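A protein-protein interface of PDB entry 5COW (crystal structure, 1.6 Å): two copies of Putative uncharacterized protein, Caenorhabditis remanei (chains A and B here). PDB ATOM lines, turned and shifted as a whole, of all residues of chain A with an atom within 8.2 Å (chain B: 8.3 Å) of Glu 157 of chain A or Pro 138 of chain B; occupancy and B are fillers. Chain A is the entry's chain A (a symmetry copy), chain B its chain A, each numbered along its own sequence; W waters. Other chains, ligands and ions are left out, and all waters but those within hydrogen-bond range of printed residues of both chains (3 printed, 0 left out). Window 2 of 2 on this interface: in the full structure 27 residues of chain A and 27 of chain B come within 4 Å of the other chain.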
ATOM      1  N   VAL A  53      14.423  -4.617  12.752  1.00  0.00           N
ATOM      2  CA  VAL A  53      13.466  -3.928  11.900  1.00  0.00           C
ATOM      3  C   VAL A  53      13.339  -2.464  12.330  1.00  0.00           C
ATOM      4  O   VAL A  53      13.332  -1.568  11.490  1.00  0.00           O
ATOM      5  CB  VAL A  53      12.080  -4.613  11.927  1.00  0.00           C
ATOM      6  CG1 VAL A  53      11.058  -3.786  11.129  1.00  0.00           C
ATOM      7  CG2 VAL A  53      12.189  -6.011  11.366  1.00  0.00           C
ATOM      8  N   SER A  56      16.480  -0.678  11.197  1.00  0.00           N
ATOM      9  CA  SER A  56      16.462  -0.429   9.756  1.00  0.00           C
ATOM     10  C   SER A  56      15.693   0.855   9.444  1.00  0.00           C
ATOM     11  O   SER A  56      16.182   1.725   8.707  1.00  0.00           O
ATOM     12  CB  SER A  56      15.842  -1.619   9.000  1.00  0.00           C
ATOM     13  OG  SER A  56      15.619  -1.263   7.640  1.00  0.00           O
ATOM     14  N   GLN A  57      14.498   0.989  10.016  1.00  0.00           N
ATOM     15  CA  GLN A  57      13.705   2.200   9.812  1.00  0.00           C
ATOM     16  C   GLN A  57      14.419   3.449  10.356  1.00  0.00           C
ATOM     17  O   GLN A  57      14.444   4.490   9.686  1.00  0.00           O
ATOM     18  CB  GLN A  57      12.321   2.065  10.454  1.00  0.00           C
ATOM     19  CG  GLN A  57      11.485   3.339  10.320  1.00  0.00           C
ATOM     20  CD  GLN A  57      10.094   3.194  10.895  1.00  0.00           C
ATOM     21  OE1 GLN A  57       9.774   2.186  11.514  1.00  0.00           O
ATOM     22  NE2 GLN A  57       9.251   4.203  10.678  1.00  0.00           N
ATOM     23  N   CYS A  60      17.020   4.651   7.955  1.00  0.00           N
ATOM     24  CA  CYS A  60      16.442   5.438   6.868  1.00  0.00           C
ATOM     25  C   CYS A  60      16.084   6.859   7.296  1.00  0.00           C
ATOM     26  O   CYS A  60      16.127   7.779   6.474  1.00  0.00           O
ATOM     27  CB  CYS A  60      15.212   4.747   6.296  1.00  0.00           C
ATOM     28  SG  CYS A  60      15.588   3.171   5.443  1.00  0.00           S
ATOM     29  N   PHE A  64      17.223  10.186   5.366  1.00  0.00           N
ATOM     30  CA  PHE A  64      16.272  11.236   4.965  1.00  0.00           C
ATOM     31  C   PHE A  64      16.870  12.618   5.279  1.00  0.00           C
ATOM     32  O   PHE A  64      16.800  13.548   4.444  1.00  0.00           O
ATOM     33  CB  PHE A  64      14.905  11.058   5.668  1.00  0.00           C
ATOM     34  CG  PHE A  64      13.950  12.232   5.479  1.00  0.00           C
ATOM     35  CD1 PHE A  64      13.959  13.306   6.366  1.00  0.00           C
ATOM     36  CD2 PHE A  64      13.026  12.242   4.433  1.00  0.00           C
ATOM     37  CE1 PHE A  64      13.092  14.383   6.200  1.00  0.00           C
ATOM     38  CE2 PHE A  64      12.151  13.325   4.266  1.00  0.00           C
ATOM     39  CZ  PHE A  64      12.181  14.382   5.154  1.00  0.00           C
ATOM     40  N   LYS A 150      20.390   4.156  -0.764  1.00  0.00           N
ATOM     41  CA  LYS A 150      19.815   4.499   0.540  1.00  0.00           C
ATOM     42  C   LYS A 150      19.277   5.934   0.583  1.00  0.00           C
ATOM     43  O   LYS A 150      18.223   6.177   1.180  1.00  0.00           O
ATOM     44  CB  LYS A 150      20.842   4.284   1.660  1.00  0.00           C
ATOM     45  CG  LYS A 150      21.078   2.810   1.999  1.00  0.00           C
ATOM     46  CD  LYS A 150      22.146   2.671   3.089  1.00  0.00           C
ATOM     47  CE  LYS A 150      22.269   1.239   3.561  1.00  0.00           C
ATOM     48  NZ  LYS A 150      23.320   1.112   4.620  1.00  0.00           N
ATOM     49  N   PHE A 151      19.981   6.877  -0.049  1.00  0.00           N
ATOM     50  CA  PHE A 151      19.511   8.276  -0.086  1.00  0.00           C
ATOM     51  C   PHE A 151      18.150   8.329  -0.782  1.00  0.00           C
ATOM     52  O   PHE A 151      17.241   9.053  -0.360  1.00  0.00           O
ATOM     53  CB  PHE A 151      20.464   9.217  -0.844  1.00  0.00           C
ATOM     54  CG  PHE A 151      21.852   9.354  -0.248  1.00  0.00           C
ATOM     55  CD1 PHE A 151      22.161   8.894   1.029  1.00  0.00           C
ATOM     56  CD2 PHE A 151      22.855   9.961  -0.992  1.00  0.00           C
ATOM     57  CE1 PHE A 151      23.450   9.027   1.540  1.00  0.00           C
ATOM     58  CE2 PHE A 151      24.138  10.096  -0.486  1.00  0.00           C
ATOM     59  CZ  PHE A 151      24.432   9.628   0.782  1.00  0.00           C
ATOM     60  N   SER A 152      18.030   7.582  -1.872  1.00  0.00           N
ATOM     61  CA  SER A 152      16.796   7.609  -2.657  1.00  0.00           C
ATOM     62  C   SER A 152      15.637   6.952  -1.906  1.00  0.00           C
ATOM     63  O   SER A 152      14.555   7.537  -1.802  1.00  0.00           O
ATOM     64  CB  SER A 152      16.994   6.917  -4.014  1.00  0.00           C
ATOM     65  OG  SER A 152      15.799   6.986  -4.787  1.00  0.00           O
ATOM     66  N   VAL A 153      15.844   5.744  -1.382  1.00  0.00           N
ATOM     67  CA  VAL A 153      14.720   5.058  -0.726  1.00  0.00           C
ATOM     68  C   VAL A 153      14.235   5.807   0.506  1.00  0.00           C
ATOM     69  O   VAL A 153      13.059   5.741   0.829  1.00  0.00           O
ATOM     70  CB  VAL A 153      15.056   3.589  -0.345  1.00  0.00           C
ATOM     71  CG1 VAL A 153      15.485   2.799  -1.579  1.00  0.00           C
ATOM     72  CG2 VAL A 153      16.091   3.515   0.745  1.00  0.00           C
ATOM     73  N   SER A 154      15.123   6.561   1.157  1.00  0.00           N
ATOM     74  CA  SER A 154      14.816   7.298   2.392  1.00  0.00           C
ATOM     75  C   SER A 154      13.819   8.429   2.177  1.00  0.00           C
ATOM     76  O   SER A 154      13.213   8.937   3.137  1.00  0.00           O
ATOM     77  CB  SER A 154      16.101   7.876   3.027  1.00  0.00           C
ATOM     78  OG  SER A 154      16.549   9.057   2.369  1.00  0.00           O
ATOM     79  N   VAL A 155      13.668   8.870   0.927  1.00  0.00           N
ATOM     80  CA  VAL A 155      12.720   9.948   0.658  1.00  0.00           C
ATOM     81  C   VAL A 155      11.481   9.455  -0.083  1.00  0.00           C
ATOM     82  O   VAL A 155      10.521  10.212  -0.284  1.00  0.00           O
ATOM     83  CB  VAL A 155      13.398  11.125  -0.114  1.00  0.00           C
ATOM     84  CG1 VAL A 155      14.540  11.664   0.713  1.00  0.00           C
ATOM     85  CG2 VAL A 155      13.883  10.703  -1.505  1.00  0.00           C
ATOM     86  N   VAL A 156      11.483   8.177  -0.445  1.00  0.00           N
ATOM     87  CA  VAL A 156      10.329   7.555  -1.085  1.00  0.00           C
ATOM     88  C   VAL A 156       9.502   6.757  -0.077  1.00  0.00           C
ATOM     89  O   VAL A 156       8.275   6.854  -0.057  1.00  0.00           O
ATOM     90  CB  VAL A 156      10.768   6.641  -2.237  1.00  0.00           C
ATOM     91  CG1 VAL A 156       9.573   5.860  -2.790  1.00  0.00           C
ATOM     92  CG2 VAL A 156      11.437   7.471  -3.335  1.00  0.00           C
ATOM     93  N   GLU A 157      10.163   5.966   0.762  1.00  0.00           N
ATOM     94  CA  GLU A 157       9.443   5.180   1.755  1.00  0.00           C
ATOM     95  C   GLU A 157       8.903   6.080   2.868  1.00  0.00           C
ATOM     96  O   GLU A 157       9.352   7.215   3.037  1.00  0.00           O
ATOM     97  CB  GLU A 157      10.351   4.087   2.344  1.00  0.00           C
ATOM     98  CG  GLU A 157      10.893   3.088   1.320  1.00  0.00           C
ATOM     99  CD  GLU A 157       9.784   2.314   0.612  1.00  0.00           C
ATOM    100  OE1 GLU A 157       8.820   1.903   1.287  1.00  0.00           O
ATOM    101  OE2 GLU A 157       9.866   2.147  -0.624  1.00  0.00           O
ATOM    102  N   LYS A 158       7.940   5.576   3.636  1.00  0.00           N
ATOM    103  CA  LYS A 158       7.422   6.342   4.768  1.00  0.00           C
ATOM    104  C   LYS A 158       8.288   6.104   6.004  1.00  0.00           C
ATOM    105  O   LYS A 158       7.995   5.231   6.824  1.00  0.00           O
ATOM    106  CB  LYS A 158       5.969   5.968   5.062  1.00  0.00           C
ATOM    107  CG  LYS A 158       5.259   6.976   5.947  1.00  0.00           C
ATOM    108  CD  LYS A 158       4.027   6.386   6.601  1.00  0.00           C
ATOM    109  CE  LYS A 158       3.343   7.414   7.483  1.00  0.00           C
ATOM    110  NZ  LYS A 158       2.313   6.799   8.374  1.00  0.00           N
ATOM    111  N   VAL A 159       9.349   6.887   6.153  1.00  0.00           N
ATOM    112  CA  VAL A 159      10.332   6.595   7.193  1.00  0.00           C
ATOM    113  C   VAL A 159       9.896   7.105   8.568  1.00  0.00           C
ATOM    114  O   VAL A 159      10.375   6.624   9.590  1.00  0.00           O
ATOM    115  CB  VAL A 159      11.733   7.171   6.833  1.00  0.00           C
ATOM    116  CG1 VAL A 159      12.152   6.719   5.431  1.00  0.00           C
ATOM    117  CG2 VAL A 159      11.767   8.689   6.939  1.00  0.00           C
ATOM    118  N   PHE A 160       8.976   8.069   8.587  1.00  0.00           N
ATOM    119  CA  PHE A 160       8.368   8.535   9.827  1.00  0.00           C
ATOM    120  C   PHE A 160       6.901   8.082   9.848  1.00  0.00           C
ATOM    121  O   PHE A 160       6.293   7.902   8.788  1.00  0.00           O
ATOM    122  CB  PHE A 160       8.460  10.068   9.951  1.00  0.00           C
ATOM    123  CG  PHE A 160       9.853  10.624   9.760  1.00  0.00           C
ATOM    124  CD1 PHE A 160      10.819  10.476  10.740  1.00  0.00           C
ATOM    125  CD2 PHE A 160      10.182  11.319   8.606  1.00  0.00           C
ATOM    126  CE1 PHE A 160      12.098  10.999  10.572  1.00  0.00           C
ATOM    127  CE2 PHE A 160      11.460  11.842   8.428  1.00  0.00           C
ATOM    128  CZ  PHE A 160      12.414  11.679   9.406  1.00  0.00           C
ATOM    129  N   VAL A 164       6.285  13.989   6.539  1.00  0.00           N
ATOM    130  CA  VAL A 164       7.210  15.091   6.744  1.00  0.00           C
ATOM    131  C   VAL A 164       7.735  15.520   5.375  1.00  0.00           C
ATOM    132  O   VAL A 164       8.377  14.723   4.693  1.00  0.00           O
ATOM    133  CB  VAL A 164       8.399  14.685   7.658  1.00  0.00           C
ATOM    134  CG1 VAL A 164       9.461  15.771   7.687  1.00  0.00           C
ATOM    135  CG2 VAL A 164       7.919  14.368   9.073  1.00  0.00           C
ATOM    136  N   ILE A 178      10.263  15.479  -4.605  1.00  0.00           N
ATOM    137  CA  ILE A 178      10.738  14.105  -4.401  1.00  0.00           C
ATOM    138  C   ILE A 178      10.979  13.407  -5.749  1.00  0.00           C
ATOM    139  O   ILE A 178      11.983  12.718  -5.930  1.00  0.00           O
ATOM    140  CB  ILE A 178       9.746  13.306  -3.539  1.00  0.00           C
ATOM    141  CG1 ILE A 178       9.832  13.804  -2.095  1.00  0.00           C
ATOM    142  CG2 ILE A 178      10.042  11.804  -3.622  1.00  0.00           C
ATOM    143  CD1 ILE A 178       8.718  13.303  -1.188  1.00  0.00           C
ATOM    144  N   THR A 182      14.623  12.082  -6.682  1.00  0.00           N
ATOM    145  CA  THR A 182      14.863  10.654  -6.910  1.00  0.00           C
ATOM    146  C   THR A 182      15.363  10.405  -8.342  1.00  0.00           C
ATOM    147  O   THR A 182      16.196   9.524  -8.547  1.00  0.00           O
ATOM    148  CB  THR A 182      13.625   9.789  -6.596  1.00  0.00           C
ATOM    149  OG1 THR A 182      12.508  10.211  -7.369  1.00  0.00           O
ATOM    150  CG2 THR A 182      13.284   9.885  -5.117  1.00  0.00           C
ATOM    151  N   LEU B  97      19.435  -5.979   9.171  1.00  0.00           N
ATOM    152  CA  LEU B  97      18.285  -6.800   8.841  1.00  0.00           C
ATOM    153  C   LEU B  97      18.595  -7.831   7.754  1.00  0.00           C
ATOM    154  O   LEU B  97      17.820  -8.772   7.544  1.00  0.00           O
ATOM    155  CB  LEU B  97      17.129  -5.890   8.413  1.00  0.00           C
ATOM    156  CG  LEU B  97      15.712  -6.441   8.322  1.00  0.00           C
ATOM    157  CD1 LEU B  97      15.273  -7.104   9.618  1.00  0.00           C
ATOM    158  CD2 LEU B  97      14.772  -5.292   7.952  1.00  0.00           C
ATOM    159  N   GLN B 133       5.089 -13.131   4.014  1.00  0.00           N
ATOM    160  CA  GLN B 133       5.051 -12.273   5.192  1.00  0.00           C
ATOM    161  C   GLN B 133       6.143 -11.213   5.119  1.00  0.00           C
ATOM    162  O   GLN B 133       5.892 -10.041   5.420  1.00  0.00           O
ATOM    163  CB  GLN B 133       5.199 -13.095   6.475  1.00  0.00           C
ATOM    164  CG  GLN B 133       5.011 -12.282   7.743  1.00  0.00           C
ATOM    165  CD  GLN B 133       5.316 -13.075   9.009  1.00  0.00           C
ATOM    166  OE1 GLN B 133       6.385 -13.677   9.143  1.00  0.00           O
ATOM    167  NE2 GLN B 133       4.371 -13.077   9.944  1.00  0.00           N
ATOM    168  N   ASP B 134       7.349 -11.611   4.702  1.00  0.00           N
ATOM    169  CA  ASP B 134       8.456 -10.653   4.589  1.00  0.00           C
ATOM    170  C   ASP B 134       8.115  -9.520   3.608  1.00  0.00           C
ATOM    171  O   ASP B 134       8.480  -8.363   3.840  1.00  0.00           O
ATOM    172  CB  ASP B 134       9.758 -11.353   4.156  1.00  0.00           C
ATOM    173  CG  ASP B 134      10.468 -12.053   5.310  1.00  0.00           C
ATOM    174  OD1 ASP B 134      10.042 -11.887   6.470  1.00  0.00           O
ATOM    175  OD2 ASP B 134      11.465 -12.773   5.063  1.00  0.00           O
ATOM    176  N   PHE B 135       7.441  -9.854   2.507  1.00  0.00           N
ATOM    177  CA  PHE B 135       7.013  -8.856   1.520  1.00  0.00           C
ATOM    178  C   PHE B 135       6.155  -7.748   2.136  1.00  0.00           C
ATOM    179  O   PHE B 135       6.139  -6.619   1.652  1.00  0.00           O
ATOM    180  CB  PHE B 135       6.202  -9.505   0.389  1.00  0.00           C
ATOM    181  CG  PHE B 135       7.023 -10.136  -0.712  1.00  0.00           C
ATOM    182  CD1 PHE B 135       8.218  -9.581  -1.142  1.00  0.00           C
ATOM    183  CD2 PHE B 135       6.559 -11.279  -1.349  1.00  0.00           C
ATOM    184  CE1 PHE B 135       8.948 -10.179  -2.179  1.00  0.00           C
ATOM    185  CE2 PHE B 135       7.278 -11.882  -2.376  1.00  0.00           C
ATOM    186  CZ  PHE B 135       8.465 -11.329  -2.800  1.00  0.00           C
ATOM    187  N   GLU B 136       5.405  -8.084   3.179  1.00  0.00           N
ATOM    188  CA  GLU B 136       4.485  -7.122   3.793  1.00  0.00           C
ATOM    189  C   GLU B 136       5.179  -5.988   4.556  1.00  0.00           C
ATOM    190  O   GLU B 136       4.558  -4.966   4.847  1.00  0.00           O
ATOM    191  CB  GLU B 136       3.517  -7.860   4.729  1.00  0.00           C
ATOM    192  CG  GLU B 136       2.583  -8.797   3.964  1.00  0.00           C
ATOM    193  CD  GLU B 136       1.728  -9.676   4.864  1.00  0.00           C
ATOM    194  OE1 GLU B 136       1.868  -9.597   6.102  1.00  0.00           O
ATOM    195  OE2 GLU B 136       0.909 -10.451   4.324  1.00  0.00           O
ATOM    196  N   CYS B 137       6.460  -6.164   4.873  1.00  0.00           N
ATOM    197  CA  CYS B 137       7.204  -5.176   5.654  1.00  0.00           C
ATOM    198  C   CYS B 137       8.132  -4.374   4.747  1.00  0.00           C
ATOM    199  O   CYS B 137       8.975  -4.966   4.074  1.00  0.00           O
ATOM    200  CB  CYS B 137       8.023  -5.860   6.753  1.00  0.00           C
ATOM    201  SG  CYS B 137       9.129  -4.741   7.653  1.00  0.00           S
ATOM    202  N   PRO B 138       7.982  -3.034   4.725  1.00  0.00           N
ATOM    203  CA  PRO B 138       8.830  -2.233   3.831  1.00  0.00           C
ATOM    204  C   PRO B 138      10.320  -2.328   4.150  1.00  0.00           C
ATOM    205  O   PRO B 138      11.136  -2.264   3.229  1.00  0.00           O
ATOM    206  CB  PRO B 138       8.330  -0.799   4.046  1.00  0.00           C
ATOM    207  CG  PRO B 138       7.573  -0.828   5.336  1.00  0.00           C
ATOM    208  CD  PRO B 138       6.988  -2.203   5.432  1.00  0.00           C
ATOM    209  N   TRP B 139      10.675  -2.480   5.423  1.00  0.00           N
ATOM    210  CA  TRP B 139      12.082  -2.511   5.810  1.00  0.00           C
ATOM    211  C   TRP B 139      12.691  -3.861   5.429  1.00  0.00           C
ATOM    212  O   TRP B 139      13.834  -3.919   4.976  1.00  0.00           O
ATOM    213  CB  TRP B 139      12.230  -2.190   7.320  1.00  0.00           C
ATOM    214  CG  TRP B 139      11.298  -1.046   7.649  1.00  0.00           C
ATOM    215  CD1 TRP B 139      10.191  -1.091   8.442  1.00  0.00           C
ATOM    216  CD2 TRP B 139      11.335   0.275   7.087  1.00  0.00           C
ATOM    217  NE1 TRP B 139       9.550   0.129   8.435  1.00  0.00           N
ATOM    218  CE2 TRP B 139      10.232   0.983   7.606  1.00  0.00           C
ATOM    219  CE3 TRP B 139      12.200   0.932   6.200  1.00  0.00           C
ATOM    220  CZ2 TRP B 139       9.970   2.310   7.273  1.00  0.00           C
ATOM    221  CZ3 TRP B 139      11.936   2.254   5.866  1.00  0.00           C
ATOM    222  CH2 TRP B 139      10.833   2.928   6.401  1.00  0.00           C
ATOM    223  N   ARG B 140      11.915  -4.938   5.572  1.00  0.00           N
ATOM    224  CA  ARG B 140      12.362  -6.240   5.083  1.00  0.00           C
ATOM    225  C   ARG B 140      12.492  -6.251   3.545  1.00  0.00           C
ATOM    226  O   ARG B 140      13.441  -6.850   3.015  1.00  0.00           O
ATOM    227  CB  ARG B 140      11.414  -7.353   5.556  1.00  0.00           C
ATOM    228  CG  ARG B 140      11.545  -7.647   7.070  1.00  0.00           C
ATOM    229  CD  ARG B 140      10.588  -8.755   7.510  1.00  0.00           C
ATOM    230  NE  ARG B 140      10.821  -9.171   8.896  1.00  0.00           N
ATOM    231  CZ  ARG B 140      10.156  -8.691   9.942  1.00  0.00           C
ATOM    232  NH1 ARG B 140       9.218  -7.766   9.768  1.00  0.00           N
ATOM    233  NH2 ARG B 140      10.432  -9.131  11.164  1.00  0.00           N
ATOM    234  N   ARG B 141      11.571  -5.585   2.841  1.00  0.00           N
ATOM    235  CA  ARG B 141      11.681  -5.463   1.377  1.00  0.00           C
ATOM    236  C   ARG B 141      12.983  -4.745   0.984  1.00  0.00           C
ATOM    237  O   ARG B 141      13.654  -5.147   0.027  1.00  0.00           O
ATOM    238  CB  ARG B 141      10.470  -4.727   0.773  1.00  0.00           C
ATOM    239  CG  ARG B 141       9.163  -5.546   0.786  1.00  0.00           C
ATOM    240  CD  ARG B 141       8.128  -5.032  -0.238  1.00  0.00           C
ATOM    241  NE  ARG B 141       7.830  -3.597  -0.104  1.00  0.00           N
ATOM    242  CZ  ARG B 141       6.925  -3.076   0.730  1.00  0.00           C
ATOM    243  NH1 ARG B 141       6.205  -3.856   1.531  1.00  0.00           N
ATOM    244  NH2 ARG B 141       6.723  -1.765   0.756  1.00  0.00           N
ATOM    245  N   LEU B 142      13.368  -3.715   1.733  1.00  0.00           N
ATOM    246  CA  LEU B 142      14.596  -3.003   1.406  1.00  0.00           C
ATOM    247  C   LEU B 142      15.805  -3.927   1.581  1.00  0.00           C
ATOM    248  O   LEU B 142      16.722  -3.911   0.757  1.00  0.00           O
ATOM    249  CB  LEU B 142      14.751  -1.733   2.267  1.00  0.00           C
ATOM    250  CG  LEU B 142      13.767  -0.592   1.949  1.00  0.00           C
ATOM    251  CD1 LEU B 142      14.062   0.590   2.853  1.00  0.00           C
ATOM    252  CD2 LEU B 142      13.852  -0.148   0.491  1.00  0.00           C
ATOM    253  N   ALA B 143      15.799  -4.733   2.644  1.00  0.00           N
ATOM    254  CA  ALA B 143      16.929  -5.608   2.957  1.00  0.00           C
ATOM    255  C   ALA B 143      17.037  -6.763   1.957  1.00  0.00           C
ATOM    256  O   ALA B 143      18.144  -7.138   1.551  1.00  0.00           O
ATOM    257  CB  ALA B 143      16.811  -6.146   4.390  1.00  0.00           C
ATOM    258  N   ILE B 144      15.896  -7.316   1.553  1.00  0.00           N
ATOM    259  CA  ILE B 144      15.886  -8.338   0.500  1.00  0.00           C
ATOM    260  C   ILE B 144      16.462  -7.770  -0.810  1.00  0.00           C
ATOM    261  O   ILE B 144      17.308  -8.401  -1.448  1.00  0.00           O
ATOM    262  CB  ILE B 144      14.470  -8.893   0.279  1.00  0.00           C
ATOM    263  CG1 ILE B 144      14.051  -9.724   1.499  1.00  0.00           C
ATOM    264  CG2 ILE B 144      14.421  -9.756  -0.991  1.00  0.00           C
ATOM    265  CD1 ILE B 144      12.553 -10.041   1.540  1.00  0.00           C
ATOM    266  N   ALA B 145      16.032  -6.571  -1.195  1.00  0.00           N
ATOM    267  CA  ALA B 145      16.583  -5.931  -2.388  1.00  0.00           C
ATOM    268  C   ALA B 145      18.103  -5.741  -2.276  1.00  0.00           C
ATOM    269  O   ALA B 145      18.840  -5.978  -3.230  1.00  0.00           O
ATOM    270  CB  ALA B 145      15.893  -4.588  -2.630  1.00  0.00           C
ATOM    271  N   VAL B 192      10.309  -7.325  -5.861  1.00  0.00           N
ATOM    272  CA  VAL B 192      10.386  -6.705  -4.541  1.00  0.00           C
ATOM    273  C   VAL B 192      10.143  -5.198  -4.605  1.00  0.00           C
ATOM    274  O   VAL B 192       9.340  -4.646  -3.839  1.00  0.00           O
ATOM    275  CB  VAL B 192      11.756  -6.978  -3.892  1.00  0.00           C
ATOM    276  CG1 VAL B 192      11.877  -6.246  -2.553  1.00  0.00           C
ATOM    277  CG2 VAL B 192      11.954  -8.481  -3.715  1.00  0.00           C
ATOM    278  N   GLU B 193      10.818  -4.531  -5.535  1.00  0.00           N
ATOM    279  CA  GLU B 193      10.764  -3.071  -5.583  1.00  0.00           C
ATOM    280  C   GLU B 193       9.435  -2.537  -6.118  1.00  0.00           C
ATOM    281  O   GLU B 193       9.072  -1.399  -5.818  1.00  0.00           O
ATOM    282  CB  GLU B 193      11.951  -2.532  -6.394  1.00  0.00           C
ATOM    283  CG  GLU B 193      13.284  -2.805  -5.665  1.00  0.00           C
ATOM    284  CD  GLU B 193      14.492  -2.057  -6.242  1.00  0.00           C
ATOM    285  OE1 GLU B 193      14.574  -1.883  -7.479  1.00  0.00           O
ATOM    286  OE2 GLU B 193      15.371  -1.647  -5.448  1.00  0.00           O
ATOM    287  N   TYR B 195       6.459  -4.227  -5.524  1.00  0.00           N
ATOM    288  CA  TYR B 195       5.425  -4.900  -4.753  1.00  0.00           C
ATOM    289  C   TYR B 195       4.182  -4.021  -4.593  1.00  0.00           C
ATOM    290  O   TYR B 195       4.272  -2.906  -4.066  1.00  0.00           O
ATOM    291  CB  TYR B 195       5.979  -5.283  -3.382  1.00  0.00           C
ATOM    292  CG  TYR B 195       4.998  -6.005  -2.482  1.00  0.00           C
ATOM    293  CD1 TYR B 195       4.592  -7.312  -2.768  1.00  0.00           C
ATOM    294  CD2 TYR B 195       4.504  -5.395  -1.334  1.00  0.00           C
ATOM    295  CE1 TYR B 195       3.707  -7.987  -1.930  1.00  0.00           C
ATOM    296  CE2 TYR B 195       3.629  -6.061  -0.493  1.00  0.00           C
ATOM    297  CZ  TYR B 195       3.232  -7.351  -0.797  1.00  0.00           C
ATOM    298  OH  TYR B 195       2.356  -8.007   0.036  1.00  0.00           O
HETATM  299  O   HOH W   1       5.750   1.085   1.267  1.00  0.00           O
HETATM  300  O   HOH W   2      10.189  -0.913   0.807  1.00  0.00           O
HETATM  301  O   HOH W   3       7.725   0.191  -1.121  1.00  0.00           O
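O of Ser 56 of chain A is in hydrogen-bond range of SG of Cys 60 of chain A (3.6 Å). SG of Cys 137 of chain B lies close to N of Trp 139 of chain B, at 3.5 Å. The side-chain carboxylate (OD1) of Asp 134 of chain B lies within salt-bridge range of the guanidinium group (NE) of Arg 140 of chain B (3.7 Å). The side-chain amide nitrogen (NE2) of Gln 57 of chain A lies within hydrogen-bond range of the backbone carbonyl oxygen (O) of Val 159 of chain A (2.9 Å). The backbone NH of Arg 140 of chain B lies within hydrogen-bond range of the side-chain sulfur of Cys 137 of chain B (3.5 Å).
Glu 157 of chain A touches just one residue of chain B: Pro 138 (3.9 Å). Pro 138 of chain B touches just one residue of chain A: Glu 157. No residue of chain A comes within 4 Å of Cys 137 of chain B. Of the printed residues of chain B, Cys 60 of chain A touches Trp 139 (3.8 Å) and Leu 142 (3.96 Å). Of the printed residues of chain A, Arg 140 of chain B touches Val 53. Of the printed residues of chain B, Val 53 of chain A touches Leu 97 (3.7 Å), Trp 139 (3.9 Å) and Arg 140 (3.6 Å). Printed residues of chain A within 4 Å of Trp 139 of chain B: Val 53 (3.9 Å), Ser 56 (3.5 Å), Gln 57 (3.6 Å), Cys 60 (3.8 Å), Lys 158 (3.6 Å) and Val 159 (3.8 Å). Ser 154 of chain A touches none of the printed residues of chain B. Ile 178 of chain A touches none of the printed residues of chain B. The nearest residue of chain A that does not touch Pro 138 of chain B is Lys 158 of chain A (6.3 Å).
Of the 19 printed residues of chain A, 8 touch a printed residue of chain B. Hydrophobic or aromatic side chains of chain A within 4 Å of the printed part of chain B: Val 53 and Val 153. Hydrophobic or aromatic side chains of chain B within 4 Å of the printed part of chain A: Leu 97, Pro 138, Trp 139 and Leu 142. Among the printed residues, 12 pairs touch across the chains. Among the printed residues, no Asp or Glu carboxylate lies within 4 Å of a Lys or Arg side-chain nitrogen of the other chain.
Water W3 lies within hydrogen-bond range of the guanidinium group of Arg 141 of chain B and the side-chain carboxylate of Glu 157 of chain A. Water W2 lies within hydrogen-bond range of O of Pro 138 of chain B (2.9 Å) and OE1 of Glu 157 of chain A (3.2 Å). Water W1 bridges the guanidinium group of Arg 141 of chain B (3.1 Å) and the side-chain carboxylate of Glu 157 of chain A (3.2 Å).
Val 53 of chain A touches Leu 97 of chain B (CG2 to CD1, 3.7 Å). Val 53 of chain A touches Trp 139 of chain B (CG1 to CD1, 3.9 Å). Val 53 of chain A touches Arg 140 of chain B (CG2 to NH2, 3.6 Å). Leu 97 of chain B touches Ser 56 of chain A. Trp 139 of chain B touches Ser 56 of chain A. SG of Cys 60 of chain A touches CZ3 of Trp 139 of chain B (3.8 Å). Leu 142 of chain B touches Cys 60 of chain A (CD1 to SG, 3.96 Å). Val 153 of chain A touches Leu 142 of chain B. Glu 157 of chain A touches Pro 138 of chain B. Val 159 of chain A touches Trp 139 of chain B.
No position is printed for both chains.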
